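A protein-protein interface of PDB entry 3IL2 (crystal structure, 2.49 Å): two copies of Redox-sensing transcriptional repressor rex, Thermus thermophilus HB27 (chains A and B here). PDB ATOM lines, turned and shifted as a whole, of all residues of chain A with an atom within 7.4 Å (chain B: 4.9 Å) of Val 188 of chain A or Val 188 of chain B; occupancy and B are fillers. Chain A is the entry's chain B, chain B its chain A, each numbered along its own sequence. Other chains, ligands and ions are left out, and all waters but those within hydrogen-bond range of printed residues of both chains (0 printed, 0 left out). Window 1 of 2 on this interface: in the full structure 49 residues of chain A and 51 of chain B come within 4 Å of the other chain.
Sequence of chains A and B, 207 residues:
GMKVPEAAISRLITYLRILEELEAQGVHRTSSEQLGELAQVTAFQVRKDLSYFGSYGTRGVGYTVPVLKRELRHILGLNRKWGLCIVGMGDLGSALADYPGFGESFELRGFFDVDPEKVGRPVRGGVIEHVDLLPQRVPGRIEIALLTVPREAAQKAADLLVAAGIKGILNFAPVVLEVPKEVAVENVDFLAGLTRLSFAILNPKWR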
ATOM      1  N   LEU A  92     -11.025   8.913 -13.609  1.00  0.00           N
ATOM      2  CA  LEU A  92     -10.515   9.216 -14.917  1.00  0.00           C
ATOM      3  C   LEU A  92     -10.999   8.144 -15.882  1.00  0.00           C
ATOM      4  O   LEU A  92     -11.476   8.410 -16.992  1.00  0.00           O
ATOM      5  CB  LEU A  92      -9.039   9.142 -14.852  1.00  0.00           C
ATOM      6  CG  LEU A  92      -8.568   9.769 -16.107  1.00  0.00           C
ATOM      7  CD1 LEU A  92      -8.785  11.240 -15.965  1.00  0.00           C
ATOM      8  CD2 LEU A  92      -7.143   9.437 -16.258  1.00  0.00           C
ATOM      9  N   LEU A 147      -4.113   2.602 -18.869  1.00  0.00           N
ATOM     10  CA  LEU A 147      -3.787   2.408 -17.487  1.00  0.00           C
ATOM     11  C   LEU A 147      -4.055   3.628 -16.619  1.00  0.00           C
ATOM     12  O   LEU A 147      -3.305   4.600 -16.663  1.00  0.00           O
ATOM     13  CB  LEU A 147      -2.337   2.038 -17.376  1.00  0.00           C
ATOM     14  CG  LEU A 147      -2.055   1.471 -16.002  1.00  0.00           C
ATOM     15  CD1 LEU A 147      -3.067   0.394 -15.699  1.00  0.00           C
ATOM     16  CD2 LEU A 147      -0.671   0.893 -15.994  1.00  0.00           C
ATOM     17  N   ILE A 169       0.475  -0.068 -23.691  1.00  0.00           N
ATOM     18  CA  ILE A 169      -0.009   0.580 -22.500  1.00  0.00           C
ATOM     19  C   ILE A 169       0.054   2.089 -22.520  1.00  0.00           C
ATOM     20  O   ILE A 169       1.142   2.669 -22.625  1.00  0.00           O
ATOM     21  CB  ILE A 169       0.789   0.144 -21.330  1.00  0.00           C
ATOM     22  CG1 ILE A 169       0.534  -1.334 -21.110  1.00  0.00           C
ATOM     23  CG2 ILE A 169       0.469   1.013 -20.131  1.00  0.00           C
ATOM     24  CD1 ILE A 169       1.459  -1.894 -20.135  1.00  0.00           C
ATOM     25  N   LEU A 170      -1.117   2.704 -22.385  1.00  0.00           N
ATOM     26  CA  LEU A 170      -1.241   4.150 -22.339  1.00  0.00           C
ATOM     27  C   LEU A 170      -1.300   4.444 -20.848  1.00  0.00           C
ATOM     28  O   LEU A 170      -2.354   4.327 -20.208  1.00  0.00           O
ATOM     29  CB  LEU A 170      -2.532   4.585 -23.025  1.00  0.00           C
ATOM     30  CG  LEU A 170      -2.788   6.091 -23.092  1.00  0.00           C
ATOM     31  CD1 LEU A 170      -1.754   6.761 -23.976  1.00  0.00           C
ATOM     32  CD2 LEU A 170      -4.183   6.340 -23.632  1.00  0.00           C
ATOM     33  N   ASN A 171      -0.154   4.831 -20.303  1.00  0.00           N
ATOM     34  CA  ASN A 171      -0.011   5.078 -18.877  1.00  0.00           C
ATOM     35  C   ASN A 171      -0.419   6.437 -18.383  1.00  0.00           C
ATOM     36  O   ASN A 171       0.117   7.450 -18.809  1.00  0.00           O
ATOM     37  CB  ASN A 171       1.437   4.825 -18.466  1.00  0.00           C
ATOM     38  CG  ASN A 171       1.622   4.835 -16.978  1.00  0.00           C
ATOM     39  OD1 ASN A 171       0.820   4.274 -16.239  1.00  0.00           O
ATOM     40  ND2 ASN A 171       2.689   5.463 -16.524  1.00  0.00           N
ATOM     41  N   PHE A 172      -1.348   6.458 -17.447  1.00  0.00           N
ATOM     42  CA  PHE A 172      -1.794   7.718 -16.906  1.00  0.00           C
ATOM     43  C   PHE A 172      -1.220   7.969 -15.559  1.00  0.00           C
ATOM     44  O   PHE A 172      -1.424   9.030 -14.983  1.00  0.00           O
ATOM     45  CB  PHE A 172      -3.284   7.734 -16.762  1.00  0.00           C
ATOM     46  CG  PHE A 172      -3.966   8.020 -18.004  1.00  0.00           C
ATOM     47  CD1 PHE A 172      -4.211   7.014 -18.925  1.00  0.00           C
ATOM     48  CD2 PHE A 172      -4.374   9.308 -18.273  1.00  0.00           C
ATOM     49  CE1 PHE A 172      -4.857   7.295 -20.099  1.00  0.00           C
ATOM     50  CE2 PHE A 172      -5.017   9.606 -19.438  1.00  0.00           C
ATOM     51  CZ  PHE A 172      -5.266   8.600 -20.359  1.00  0.00           C
ATOM     52  N   ALA A 173      -0.533   6.962 -15.042  1.00  0.00           N
ATOM     53  CA  ALA A 173       0.072   7.035 -13.729  1.00  0.00           C
ATOM     54  C   ALA A 173       1.408   7.721 -13.826  1.00  0.00           C
ATOM     55  O   ALA A 173       2.185   7.470 -14.750  1.00  0.00           O
ATOM     56  CB  ALA A 173       0.246   5.643 -13.160  1.00  0.00           C
ATOM     57  N   PRO A 174       1.698   8.609 -12.864  1.00  0.00           N
ATOM     58  CA  PRO A 174       2.949   9.367 -12.796  1.00  0.00           C
ATOM     59  C   PRO A 174       4.106   8.542 -12.268  1.00  0.00           C
ATOM     60  O   PRO A 174       4.406   8.580 -11.075  1.00  0.00           O
ATOM     61  CB  PRO A 174       2.609  10.529 -11.877  1.00  0.00           C
ATOM     62  CG  PRO A 174       1.599   9.936 -10.944  1.00  0.00           C
ATOM     63  CD  PRO A 174       0.749   9.048 -11.825  1.00  0.00           C
ATOM     64  N   GLU A 186       3.268   4.506 -23.621  1.00  0.00           N
ATOM     65  CA  GLU A 186       3.195   5.935 -23.860  1.00  0.00           C
ATOM     66  C   GLU A 186       2.630   6.555 -22.606  1.00  0.00           C
ATOM     67  O   GLU A 186       1.679   6.039 -22.020  1.00  0.00           O
ATOM     68  CB  GLU A 186       2.279   6.241 -25.046  1.00  0.00           C
ATOM     69  CG  GLU A 186       2.920   6.064 -26.415  1.00  0.00           C
ATOM     70  CD  GLU A 186       4.082   7.018 -26.638  1.00  0.00           C
ATOM     71  OE1 GLU A 186       3.910   8.227 -26.372  1.00  0.00           O
ATOM     72  OE2 GLU A 186       5.162   6.567 -27.082  1.00  0.00           O
ATOM     73  N   ASN A 187       3.218   7.663 -22.187  1.00  0.00           N
ATOM     74  CA  ASN A 187       2.731   8.309 -20.999  1.00  0.00           C
ATOM     75  C   ASN A 187       1.878   9.510 -21.303  1.00  0.00           C
ATOM     76  O   ASN A 187       2.120  10.248 -22.253  1.00  0.00           O
ATOM     77  CB  ASN A 187       3.878   8.764 -20.113  1.00  0.00           C
ATOM     78  CG  ASN A 187       4.765   7.629 -19.676  1.00  0.00           C
ATOM     79  OD1 ASN A 187       4.289   6.599 -19.188  1.00  0.00           O
ATOM     80  ND2 ASN A 187       6.073   7.813 -19.835  1.00  0.00           N
ATOM     81  N   VAL A 188       0.846   9.671 -20.505  1.00  0.00           N
ATOM     82  CA  VAL A 188      -0.001  10.831 -20.597  1.00  0.00           C
ATOM     83  C   VAL A 188       0.072  11.326 -19.166  1.00  0.00           C
ATOM     84  O   VAL A 188      -0.573  10.790 -18.270  1.00  0.00           O
ATOM     85  CB  VAL A 188      -1.420  10.482 -20.944  1.00  0.00           C
ATOM     86  CG1 VAL A 188      -2.178  11.750 -21.190  1.00  0.00           C
ATOM     87  CG2 VAL A 188      -1.448   9.640 -22.176  1.00  0.00           C
ATOM     88  N   ASP A 189       0.871  12.358 -18.961  1.00  0.00           N
ATOM     89  CA  ASP A 189       1.123  12.844 -17.616  1.00  0.00           C
ATOM     90  C   ASP A 189       0.745  14.295 -17.423  1.00  0.00           C
ATOM     91  O   ASP A 189       1.518  15.191 -17.752  1.00  0.00           O
ATOM     92  CB  ASP A 189       2.606  12.610 -17.343  1.00  0.00           C
ATOM     93  CG  ASP A 189       2.985  12.805 -15.899  1.00  0.00           C
ATOM     94  OD1 ASP A 189       4.073  12.318 -15.527  1.00  0.00           O
ATOM     95  OD2 ASP A 189       2.233  13.443 -15.140  1.00  0.00           O
ATOM     96  N   PHE A 190      -0.427  14.529 -16.846  1.00  0.00           N
ATOM     97  CA  PHE A 190      -0.889  15.887 -16.690  1.00  0.00           C
ATOM     98  C   PHE A 190      -0.165  16.648 -15.597  1.00  0.00           C
ATOM     99  O   PHE A 190       0.019  17.862 -15.691  1.00  0.00           O
ATOM    100  CB  PHE A 190      -2.413  15.907 -16.539  1.00  0.00           C
ATOM    101  CG  PHE A 190      -2.881  15.917 -15.149  1.00  0.00           C
ATOM    102  CD1 PHE A 190      -2.835  17.085 -14.404  1.00  0.00           C
ATOM    103  CD2 PHE A 190      -3.401  14.770 -14.580  1.00  0.00           C
ATOM    104  CE1 PHE A 190      -3.280  17.108 -13.110  1.00  0.00           C
ATOM    105  CE2 PHE A 190      -3.862  14.780 -13.288  1.00  0.00           C
ATOM    106  CZ  PHE A 190      -3.801  15.955 -12.548  1.00  0.00           C
ATOM    107  N   LEU A 191       0.277  15.942 -14.570  1.00  0.00           N
ATOM    108  CA  LEU A 191       1.037  16.598 -13.529  1.00  0.00           C
ATOM    109  C   LEU A 191       2.414  17.001 -14.049  1.00  0.00           C
ATOM    110  O   LEU A 191       2.971  18.017 -13.620  1.00  0.00           O
ATOM    111  CB  LEU A 191       1.221  15.679 -12.364  1.00  0.00           C
ATOM    112  CG  LEU A 191      -0.010  15.646 -11.497  1.00  0.00           C
ATOM    113  CD1 LEU A 191       0.263  14.728 -10.387  1.00  0.00           C
ATOM    114  CD2 LEU A 191      -0.298  16.999 -10.926  1.00  0.00           C
ATOM    115  N   ALA A 192       2.985  16.206 -14.950  1.00  0.00           N
ATOM    116  CA  ALA A 192       4.292  16.570 -15.473  1.00  0.00           C
ATOM    117  C   ALA A 192       4.107  17.859 -16.260  1.00  0.00           C
ATOM    118  O   ALA A 192       4.920  18.781 -16.153  1.00  0.00           O
ATOM    119  CB  ALA A 192       4.852  15.469 -16.366  1.00  0.00           C
ATOM    120  N   GLY A 193       3.019  17.920 -17.034  1.00  0.00           N
ATOM    121  CA  GLY A 193       2.713  19.105 -17.828  1.00  0.00           C
ATOM    122  C   GLY A 193       2.531  20.342 -16.958  1.00  0.00           C
ATOM    123  O   GLY A 193       2.969  21.437 -17.319  1.00  0.00           O
ATOM    124  N   LEU A 194       1.864  20.181 -15.823  1.00  0.00           N
ATOM    125  CA  LEU A 194       1.694  21.280 -14.891  1.00  0.00           C
ATOM    126  C   LEU A 194       3.021  21.781 -14.424  1.00  0.00           C
ATOM    127  O   LEU A 194       3.257  22.983 -14.360  1.00  0.00           O
ATOM    128  CB  LEU A 194       1.020  20.840 -13.621  1.00  0.00           C
ATOM    129  CG  LEU A 194      -0.470  20.849 -13.645  1.00  0.00           C
ATOM    130  CD1 LEU A 194      -0.934  20.735 -12.223  1.00  0.00           C
ATOM    131  CD2 LEU A 194      -0.948  22.144 -14.249  1.00  0.00           C
ATOM    132  N   ARG A 196       5.838  21.386 -15.808  1.00  0.00           N
ATOM    133  CA  ARG A 196       6.499  22.077 -16.885  1.00  0.00           C
ATOM    134  C   ARG A 196       5.971  23.481 -17.070  1.00  0.00           C
ATOM    135  O   ARG A 196       6.688  24.367 -17.538  1.00  0.00           O
ATOM    136  CB  ARG A 196       6.300  21.353 -18.176  1.00  0.00           C
ATOM    137  CG  ARG A 196       7.102  20.126 -18.213  1.00  0.00           C
ATOM    138  CD  ARG A 196       7.320  19.757 -19.638  1.00  0.00           C
ATOM    139  NE  ARG A 196       6.144  19.078 -20.140  1.00  0.00           N
ATOM    140  CZ  ARG A 196       5.811  17.848 -19.769  1.00  0.00           C
ATOM    141  NH1 ARG A 196       6.581  17.181 -18.904  1.00  0.00           N
ATOM    142  NH2 ARG A 196       4.706  17.289 -20.248  1.00  0.00           N
ATOM    143  N   LEU B 170      -2.747  24.666 -19.565  1.00  0.00           N
ATOM    144  CA  LEU B 170      -2.477  23.239 -19.630  1.00  0.00           C
ATOM    145  C   LEU B 170      -3.629  22.803 -20.518  1.00  0.00           C
ATOM    146  O   LEU B 170      -4.773  22.637 -20.054  1.00  0.00           O
ATOM    147  CB  LEU B 170      -2.581  22.578 -18.256  1.00  0.00           C
ATOM    148  CG  LEU B 170      -2.204  21.086 -18.227  1.00  0.00           C
ATOM    149  CD1 LEU B 170      -0.818  20.851 -18.852  1.00  0.00           C
ATOM    150  CD2 LEU B 170      -2.199  20.604 -16.790  1.00  0.00           C
ATOM    151  N   ASN B 171      -3.323  22.646 -21.801  1.00  0.00           N
ATOM    152  CA  ASN B 171      -4.306  22.283 -22.830  1.00  0.00           C
ATOM    153  C   ASN B 171      -4.566  20.795 -22.990  1.00  0.00           C
ATOM    154  O   ASN B 171      -3.661  20.047 -23.329  1.00  0.00           O
ATOM    155  CB  ASN B 171      -3.850  22.853 -24.172  1.00  0.00           C
ATOM    156  CG  ASN B 171      -4.767  22.493 -25.285  1.00  0.00           C
ATOM    157  OD1 ASN B 171      -5.974  22.417 -25.103  1.00  0.00           O
ATOM    158  ND2 ASN B 171      -4.206  22.286 -26.465  1.00  0.00           N
ATOM    159  N   PHE B 172      -5.812  20.388 -22.761  1.00  0.00           N
ATOM    160  CA  PHE B 172      -6.225  18.992 -22.882  1.00  0.00           C
ATOM    161  C   PHE B 172      -6.998  18.756 -24.182  1.00  0.00           C
ATOM    162  O   PHE B 172      -7.443  17.636 -24.450  1.00  0.00           O
ATOM    163  CB  PHE B 172      -7.138  18.567 -21.714  1.00  0.00           C
ATOM    164  CG  PHE B 172      -6.467  18.537 -20.371  1.00  0.00           C
ATOM    165  CD1 PHE B 172      -6.218  19.714 -19.674  1.00  0.00           C
ATOM    166  CD2 PHE B 172      -6.149  17.324 -19.777  1.00  0.00           C
ATOM    167  CE1 PHE B 172      -5.670  19.682 -18.400  1.00  0.00           C
ATOM    168  CE2 PHE B 172      -5.598  17.268 -18.489  1.00  0.00           C
ATOM    169  CZ  PHE B 172      -5.356  18.450 -17.796  1.00  0.00           C
ATOM    170  N   GLU B 186       1.122  23.946 -22.413  1.00  0.00           N
ATOM    171  CA  GLU B 186       1.569  22.573 -22.285  1.00  0.00           C
ATOM    172  C   GLU B 186       0.369  21.736 -22.641  1.00  0.00           C
ATOM    173  O   GLU B 186      -0.730  21.979 -22.155  1.00  0.00           O
ATOM    174  CB  GLU B 186       1.987  22.251 -20.861  1.00  0.00           C
ATOM    175  CG  GLU B 186       3.391  22.635 -20.516  1.00  0.00           C
ATOM    176  CD  GLU B 186       4.392  21.928 -21.386  1.00  0.00           C
ATOM    177  OE1 GLU B 186       4.305  20.686 -21.512  1.00  0.00           O
ATOM    178  OE2 GLU B 186       5.273  22.615 -21.946  1.00  0.00           O
ATOM    179  N   ASN B 187       0.575  20.738 -23.479  1.00  0.00           N
ATOM    180  CA  ASN B 187      -0.515  19.878 -23.888  1.00  0.00           C
ATOM    181  C   ASN B 187      -0.473  18.516 -23.222  1.00  0.00           C
ATOM    182  O   ASN B 187       0.583  17.966 -22.983  1.00  0.00           O
ATOM    183  CB  ASN B 187      -0.466  19.654 -25.397  1.00  0.00           C
ATOM    184  CG  ASN B 187      -0.560  20.934 -26.191  1.00  0.00           C
ATOM    185  OD1 ASN B 187      -1.561  21.651 -26.127  1.00  0.00           O
ATOM    186  ND2 ASN B 187       0.481  21.227 -26.956  1.00  0.00           N
ATOM    187  N   VAL B 188      -1.644  17.994 -22.899  1.00  0.00           N
ATOM    188  CA  VAL B 188      -1.773  16.654 -22.363  1.00  0.00           C
ATOM    189  C   VAL B 188      -2.754  16.072 -23.365  1.00  0.00           C
ATOM    190  O   VAL B 188      -3.956  16.334 -23.305  1.00  0.00           O
ATOM    191  CB  VAL B 188      -2.383  16.615 -20.983  1.00  0.00           C
ATOM    192  CG1 VAL B 188      -2.708  15.171 -20.637  1.00  0.00           C
ATOM    193  CG2 VAL B 188      -1.396  17.204 -19.962  1.00  0.00           C
ATOM    194  N   ASP B 189      -2.215  15.294 -24.297  1.00  0.00           N
ATOM    195  CA  ASP B 189      -2.978  14.730 -25.400  1.00  0.00           C
ATOM    196  C   ASP B 189      -3.006  13.197 -25.362  1.00  0.00           C
ATOM    197  O   ASP B 189      -2.093  12.537 -25.877  1.00  0.00           O
ATOM    198  CB  ASP B 189      -2.315  15.262 -26.684  1.00  0.00           C
ATOM    199  CG  ASP B 189      -3.181  15.130 -27.915  1.00  0.00           C
ATOM    200  OD1 ASP B 189      -2.762  15.674 -28.966  1.00  0.00           O
ATOM    201  OD2 ASP B 189      -4.254  14.486 -27.850  1.00  0.00           O
ATOM    202  N   PHE B 190      -4.056  12.629 -24.769  1.00  0.00           N
ATOM    203  CA  PHE B 190      -4.155  11.174 -24.677  1.00  0.00           C
ATOM    204  C   PHE B 190      -4.545  10.539 -26.008  1.00  0.00           C
ATOM    205  O   PHE B 190      -4.131   9.424 -26.299  1.00  0.00           O
ATOM    206  CB  PHE B 190      -5.121  10.738 -23.558  1.00  0.00           C
ATOM    207  CG  PHE B 190      -6.563  10.670 -23.982  1.00  0.00           C
ATOM    208  CD1 PHE B 190      -7.377  11.808 -23.938  1.00  0.00           C
ATOM    209  CD2 PHE B 190      -7.100   9.470 -24.469  1.00  0.00           C
ATOM    210  CE1 PHE B 190      -8.709  11.752 -24.381  1.00  0.00           C
ATOM    211  CE2 PHE B 190      -8.422   9.399 -24.913  1.00  0.00           C
ATOM    212  CZ  PHE B 190      -9.231  10.541 -24.874  1.00  0.00           C
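OE1 of Glu 186 of chain B lies within salt-bridge range of NE of Arg 196 of chain A.
Of chain B, only Val 188 (3.5 Å) and Phe 190 (3.9 Å) come within 4 Å of Val 188 of chain A.
Of chain A, only Val 188 and Phe 190 come within 4 Å of Val 188 of chain B.
Of the printed residues of chain A, Phe 190 of chain B touches Phe 172 and Val 188.
Of the printed residues of chain A, Glu 186 of chain B touches Gly 193 (3.4 Å) and Arg 196 (2.8 Å).
Of the printed residues of chain B, Arg 196 of chain A touches Glu 186.
Of the printed residues of chain A, Leu 170 of chain B touches Phe 190, Gly 193 and Leu 194.
Printed residues of chain A within 4 Å of Phe 172 of chain B: Phe 190.
Leu 92 of chain A touches none of the printed residues of chain B.
Asn 171 of chain B touches none of the printed residues of chain A.
The nearest residue of chain A that does not touch Val 188 of chain B is Asp 189 of chain A (4.2 Å).
The nearest printed residue of chain A that does not touch Glu 186 of chain B is Leu 194 of chain A (5.4 Å).
Phe 172 of chain A touches Phe 190 of chain B, and with the chains exchanged Phe 190 of chain A touches Phe 172 of chain B.
Val 188 of chain A touches its own counterpart, Val 188 of chain B.
Val 188 of chain A touches Phe 190 of chain B, and with the chains exchanged Phe 190 of chain A touches Val 188 of chain B.
Phe 190 of chain A touches Leu 170 of chain B, but with the chains exchanged Leu 170 of chain A does not touch Phe 190 of chain B (4.1 Å).
O of Asn 171 of chain B sits at hydrogen-bond distance from N of Val 188 of chain B (2.9 Å).
N of Asn 171 of chain B sits at hydrogen-bond distance from O of Glu 186 of chain B.
N of Phe 172 of chain A lies within hydrogen-bond range of O of Leu 147 of chain A.
The backbone carbonyl oxygen (O) of Asn 171 of chain A sits at hydrogen-bond distance from the backbone NH (N) of Val 188 of chain A (2.9 Å).
Among the printed residues, pairs that only touch across the chains: Leu 194 of chain A with Leu 170 of chain B, Gly 193 of chain A with Glu 186 of chain B, Val 188 of chain A with Val 188 of chain B, Phe 190 of chain A with Val 188 of chain B, Phe 190 of chain A with Leu 170 of chain B, Phe 172 of chain A with Phe 190 of chain B, Gly 193 of chain A with Leu 170 of chain B, Val 188 of chain A with Phe 190 of chain B and Phe 190 of chain A with Phe 172 of chain B.
Printed residues of chain A that touch a printed residue of chain B: Phe 172, Val 188, Phe 190, Gly 193, Leu 194 and Arg 196.
Hydrophobic or aromatic side chains of chain A that line the printed part of chain B: Phe 172, Val 188, Phe 190 and Leu 194.
Along chain A the printed residues that touch a printed residue of chain B span positions 172 to 196.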
